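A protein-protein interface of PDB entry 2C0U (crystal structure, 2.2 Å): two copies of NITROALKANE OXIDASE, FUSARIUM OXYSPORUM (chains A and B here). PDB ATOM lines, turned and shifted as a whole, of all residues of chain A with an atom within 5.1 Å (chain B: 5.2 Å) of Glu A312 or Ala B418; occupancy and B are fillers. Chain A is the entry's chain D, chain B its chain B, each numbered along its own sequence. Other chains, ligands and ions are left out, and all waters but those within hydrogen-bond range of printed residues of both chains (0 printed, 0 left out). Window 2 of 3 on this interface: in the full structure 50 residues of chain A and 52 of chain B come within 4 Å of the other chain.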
ATOM      1  N   LYS A 300      -8.456  21.173  -6.043  1.00  0.00           N
ATOM      2  CA  LYS A 300      -9.102  22.458  -5.831  1.00  0.00           C
ATOM      3  C   LYS A 300      -9.734  22.994  -7.111  1.00  0.00           C
ATOM      4  O   LYS A 300     -10.298  24.085  -7.120  1.00  0.00           O
ATOM      5  CB  LYS A 300      -8.091  23.462  -5.276  1.00  0.00           C
ATOM      6  CG  LYS A 300      -7.577  23.087  -3.900  1.00  0.00           C
ATOM      7  CD  LYS A 300      -6.403  23.950  -3.500  1.00  0.00           C
ATOM      8  CE  LYS A 300      -6.816  25.381  -3.190  1.00  0.00           C
ATOM      9  NZ  LYS A 300      -5.604  26.190  -2.884  1.00  0.00           N
ATOM     10  N   LYS A 308     -19.058  19.569  -5.740  1.00  0.00           N
ATOM     11  CA  LYS A 308     -17.985  20.393  -5.178  1.00  0.00           C
ATOM     12  C   LYS A 308     -16.587  19.838  -5.453  1.00  0.00           C
ATOM     13  O   LYS A 308     -16.423  18.664  -5.767  1.00  0.00           O
ATOM     14  CB  LYS A 308     -18.170  20.537  -3.668  1.00  0.00           C
ATOM     15  CG  LYS A 308     -18.139  19.227  -2.922  1.00  0.00           C
ATOM     16  CD  LYS A 308     -18.524  19.417  -1.472  1.00  0.00           C
ATOM     17  CE  LYS A 308     -18.360  18.120  -0.699  1.00  0.00           C
ATOM     18  NZ  LYS A 308     -18.774  18.259   0.723  1.00  0.00           N
ATOM     19  N   HIS A 309     -15.584  20.700  -5.338  1.00  0.00           N
ATOM     20  CA  HIS A 309     -14.193  20.301  -5.534  1.00  0.00           C
ATOM     21  C   HIS A 309     -13.878  19.131  -4.605  1.00  0.00           C
ATOM     22  O   HIS A 309     -14.263  19.143  -3.434  1.00  0.00           O
ATOM     23  CB  HIS A 309     -13.285  21.481  -5.218  1.00  0.00           C
ATOM     24  CG  HIS A 309     -13.476  22.643  -6.139  1.00  0.00           C
ATOM     25  ND1 HIS A 309     -13.127  23.930  -5.791  1.00  0.00           N
ATOM     26  CD2 HIS A 309     -13.965  22.712  -7.397  1.00  0.00           C
ATOM     27  CE1 HIS A 309     -13.396  24.742  -6.799  1.00  0.00           C
ATOM     28  NE2 HIS A 309     -13.905  24.026  -7.786  1.00  0.00           N
ATOM     29  N   ILE A 310     -13.167  18.129  -5.115  1.00  0.00           N
ATOM     30  CA  ILE A 310     -12.869  16.941  -4.316  1.00  0.00           C
ATOM     31  C   ILE A 310     -12.125  17.220  -3.017  1.00  0.00           C
ATOM     32  O   ILE A 310     -12.194  16.426  -2.074  1.00  0.00           O
ATOM     33  CB  ILE A 310     -12.102  15.898  -5.137  1.00  0.00           C
ATOM     34  CG1 ILE A 310     -10.813  16.507  -5.675  1.00  0.00           C
ATOM     35  CG2 ILE A 310     -12.992  15.384  -6.268  1.00  0.00           C
ATOM     36  CD1 ILE A 310      -9.867  15.482  -6.191  1.00  0.00           C
ATOM     37  N   ILE A 311     -11.433  18.351  -2.951  1.00  0.00           N
ATOM     38  CA  ILE A 311     -10.726  18.702  -1.733  1.00  0.00           C
ATOM     39  C   ILE A 311     -11.709  18.899  -0.564  1.00  0.00           C
ATOM     40  O   ILE A 311     -11.317  18.867   0.603  1.00  0.00           O
ATOM     41  CB  ILE A 311      -9.872  19.970  -1.922  1.00  0.00           C
ATOM     42  CG1 ILE A 311      -8.901  20.086  -0.752  1.00  0.00           C
ATOM     43  CG2 ILE A 311     -10.761  21.216  -2.019  1.00  0.00           C
ATOM     44  CD1 ILE A 311      -7.758  20.994  -1.028  1.00  0.00           C
ATOM     45  N   GLU A 312     -12.989  19.088  -0.882  1.00  0.00           N
ATOM     46  CA  GLU A 312     -14.017  19.257   0.143  1.00  0.00           C
ATOM     47  C   GLU A 312     -14.364  17.899   0.749  1.00  0.00           C
ATOM     48  O   GLU A 312     -15.078  17.817   1.750  1.00  0.00           O
ATOM     49  CB  GLU A 312     -15.268  19.897  -0.459  1.00  0.00           C
ATOM     50  CG  GLU A 312     -14.977  21.163  -1.247  1.00  0.00           C
ATOM     51  CD  GLU A 312     -14.440  22.292  -0.385  1.00  0.00           C
ATOM     52  OE1 GLU A 312     -13.894  23.264  -0.958  1.00  0.00           O
ATOM     53  OE2 GLU A 312     -14.572  22.221   0.860  1.00  0.00           O
ATOM     54  N   HIS A 313     -13.876  16.823   0.141  1.00  0.00           N
ATOM     55  CA  HIS A 313     -14.137  15.492   0.690  1.00  0.00           C
ATOM     56  C   HIS A 313     -13.065  15.210   1.737  1.00  0.00           C
ATOM     57  O   HIS A 313     -11.878  15.291   1.443  1.00  0.00           O
ATOM     58  CB  HIS A 313     -14.075  14.429  -0.408  1.00  0.00           C
ATOM     59  CG  HIS A 313     -15.116  14.599  -1.469  1.00  0.00           C
ATOM     60  ND1 HIS A 313     -16.464  14.629  -1.193  1.00  0.00           N
ATOM     61  CD2 HIS A 313     -15.002  14.754  -2.810  1.00  0.00           C
ATOM     62  CE1 HIS A 313     -17.137  14.798  -2.314  1.00  0.00           C
ATOM     63  NE2 HIS A 313     -16.276  14.875  -3.313  1.00  0.00           N
ATOM     64  N   GLN A 314     -13.473  14.876   2.954  1.00  0.00           N
ATOM     65  CA  GLN A 314     -12.496  14.623   4.007  1.00  0.00           C
ATOM     66  C   GLN A 314     -11.421  13.603   3.630  1.00  0.00           C
ATOM     67  O   GLN A 314     -10.236  13.828   3.899  1.00  0.00           O
ATOM     68  CB  GLN A 314     -13.189  14.189   5.301  1.00  0.00           C
ATOM     69  CG  GLN A 314     -14.099  15.270   5.892  1.00  0.00           C
ATOM     70  CD  GLN A 314     -14.632  14.910   7.269  1.00  0.00           C
ATOM     71  OE1 GLN A 314     -14.602  13.749   7.686  1.00  0.00           O
ATOM     72  NE2 GLN A 314     -15.136  15.910   7.980  1.00  0.00           N
ATOM     73  N   MET B 413      -7.593  22.489   9.066  1.00  0.00           N
ATOM     74  CA  MET B 413      -6.539  22.534   8.062  1.00  0.00           C
ATOM     75  C   MET B 413      -7.121  22.366   6.671  1.00  0.00           C
ATOM     76  O   MET B 413      -6.703  23.030   5.728  1.00  0.00           O
ATOM     77  CB  MET B 413      -5.492  21.450   8.334  1.00  0.00           C
ATOM     78  CG  MET B 413      -4.119  21.803   7.790  1.00  0.00           C
ATOM     79  SD  MET B 413      -2.794  20.438   8.140  1.00  0.00           S
ATOM     80  CE  MET B 413      -1.848  20.662   6.497  1.00  0.00           C
ATOM     81  N   GLN B 414      -8.081  21.461   6.543  1.00  0.00           N
ATOM     82  CA  GLN B 414      -8.732  21.231   5.260  1.00  0.00           C
ATOM     83  C   GLN B 414      -9.341  22.548   4.757  1.00  0.00           C
ATOM     84  O   GLN B 414      -9.226  22.895   3.578  1.00  0.00           O
ATOM     85  CB  GLN B 414      -9.836  20.181   5.432  1.00  0.00           C
ATOM     86  CG  GLN B 414     -10.613  19.868   4.164  1.00  0.00           C
ATOM     87  CD  GLN B 414     -11.720  18.835   4.372  1.00  0.00           C
ATOM     88  OE1 GLN B 414     -12.469  18.524   3.445  1.00  0.00           O
ATOM     89  NE2 GLN B 414     -11.819  18.294   5.583  1.00  0.00           N
ATOM     90  N   ARG B 415      -9.981  23.280   5.666  1.00  0.00           N
ATOM     91  CA  ARG B 415     -10.626  24.543   5.328  1.00  0.00           C
ATOM     92  C   ARG B 415      -9.607  25.516   4.751  1.00  0.00           C
ATOM     93  O   ARG B 415      -9.826  26.105   3.695  1.00  0.00           O
ATOM     94  CB  ARG B 415     -11.273  25.145   6.576  1.00  0.00           C
ATOM     95  CG  ARG B 415     -12.433  26.094   6.314  1.00  0.00           C
ATOM     96  CD  ARG B 415     -12.723  26.948   7.547  1.00  0.00           C
ATOM     97  NE  ARG B 415     -12.632  26.200   8.804  1.00  0.00           N
ATOM     98  CZ  ARG B 415     -13.401  25.164   9.132  1.00  0.00           C
ATOM     99  NH1 ARG B 415     -14.339  24.733   8.299  1.00  0.00           N
ATOM    100  NH2 ARG B 415     -13.230  24.553  10.298  1.00  0.00           N
ATOM    101  N   VAL B 416      -8.486  25.667   5.446  1.00  0.00           N
ATOM    102  CA  VAL B 416      -7.423  26.568   5.019  1.00  0.00           C
ATOM    103  C   VAL B 416      -6.888  26.225   3.636  1.00  0.00           C
ATOM    104  O   VAL B 416      -6.646  27.115   2.816  1.00  0.00           O
ATOM    105  CB  VAL B 416      -6.248  26.538   6.016  1.00  0.00           C
ATOM    106  CG1 VAL B 416      -5.091  27.348   5.488  1.00  0.00           C
ATOM    107  CG2 VAL B 416      -6.694  27.089   7.348  1.00  0.00           C
ATOM    108  N   MET B 417      -6.701  24.931   3.388  1.00  0.00           N
ATOM    109  CA  MET B 417      -6.172  24.456   2.110  1.00  0.00           C
ATOM    110  C   MET B 417      -7.189  24.658   0.997  1.00  0.00           C
ATOM    111  O   MET B 417      -6.825  24.878  -0.150  1.00  0.00           O
ATOM    112  CB  MET B 417      -5.803  22.961   2.192  1.00  0.00           C
ATOM    113  CG  MET B 417      -4.795  22.576   3.284  1.00  0.00           C
ATOM    114  SD  MET B 417      -4.413  20.672   3.332  1.00  0.00           S
ATOM    115  CE  MET B 417      -3.104  20.631   1.929  1.00  0.00           C
ATOM    116  N   ALA B 418      -8.468  24.573   1.339  1.00  0.00           N
ATOM    117  CA  ALA B 418      -9.526  24.752   0.354  1.00  0.00           C
ATOM    118  C   ALA B 418      -9.581  26.192  -0.179  1.00  0.00           C
ATOM    119  O   ALA B 418     -10.063  26.427  -1.285  1.00  0.00           O
ATOM    120  CB  ALA B 418     -10.865  24.367   0.961  1.00  0.00           C
ATOM    121  N   LEU B 419      -9.090  27.149   0.606  1.00  0.00           N
ATOM    122  CA  LEU B 419      -9.099  28.555   0.197  1.00  0.00           C
ATOM    123  C   LEU B 419      -8.408  28.754  -1.144  1.00  0.00           C
ATOM    124  O   LEU B 419      -7.422  28.087  -1.448  1.00  0.00           O
ATOM    125  CB  LEU B 419      -8.417  29.429   1.252  1.00  0.00           C
ATOM    126  CG  LEU B 419      -9.140  29.524   2.596  1.00  0.00           C
ATOM    127  CD1 LEU B 419      -8.327  30.349   3.585  1.00  0.00           C
ATOM    128  CD2 LEU B 419     -10.505  30.148   2.373  1.00  0.00           C
ATOM    129  N   GLU B 420      -8.924  29.685  -1.937  1.00  0.00           N
ATOM    130  CA  GLU B 420      -8.368  29.977  -3.255  1.00  0.00           C
ATOM    131  C   GLU B 420      -6.978  30.608  -3.205  1.00  0.00           C
ATOM    132  O   GLU B 420      -6.169  30.421  -4.113  1.00  0.00           O
ATOM    133  CB  GLU B 420      -9.323  30.896  -4.016  1.00  0.00           C
ATOM    134  CG  GLU B 420      -8.826  31.331  -5.380  1.00  0.00           C
ATOM    135  CD  GLU B 420      -9.823  32.218  -6.101  1.00  0.00           C
ATOM    136  OE1 GLU B 420      -9.476  32.750  -7.176  1.00  0.00           O
ATOM    137  OE2 GLU B 420     -10.957  32.383  -5.597  1.00  0.00           O
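Among the printed residues, merely in contact across the chains: Lys A300 with Ala B418 (3.9 Å), Glu A312 with Ala B418 (3.8 Å), His A313 with Gln B414 (3.8 Å) and Gln A314 with Gln B414 (3.8 Å).
OE1 of Gln B414 sits close to O of Ile A311, at 3.1 Å.
NZ of Lys A300 lies close to O of Met B417 (3.3 Å).
O of Glu A312 lies close to OE1 of Gln B414 (3.2 Å).
The side-chain amino group of Lys A300 lies within hydrogen-bond range of the backbone carbonyl oxygen of Leu B419 (3.0 Å).
The backbone carbonyl oxygen (O) of Lys A300 is in hydrogen-bond range of a ring nitrogen (ND1) of His A309 (3.1 Å).
Hydrophobic or aromatic side chains of chain B within 4 Å of the printed part of chain A: Ala B418.
Of the 8 printed residues of chain A, 5 touch a printed residue of chain B.
Printed residues of chain A that touch a printed residue of chain B: Lys A300, Ile A311, Glu A312, His A313 and Gln A314.
No position is printed for both chains.
Of the 8 pairs that touch across the chains among the printed residues, none has its exchanged pair printed and touching as well.
Printed residues of chain B within 4 Å of Lys A300: Met B417 (3.1 Å), Ala B418 (3.9 Å) and Leu B419 (3.0 Å).
Glu A312 touches just these residues of chain B: Gln B414 (3.2 Å) and Ala B418 (3.8 Å).
Of the printed residues of chain B, His A313 touches Gln B414 (3.8 Å).
Met B413 touches none of the printed residues of chain A.
Arg B415 touches none of the printed residues of chain A.
Of the printed residues of chain A, Met B417 touches Lys A300.
The nearest printed residue of chain B that does not touch Glu A312 is Leu B419 (6.4 Å).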
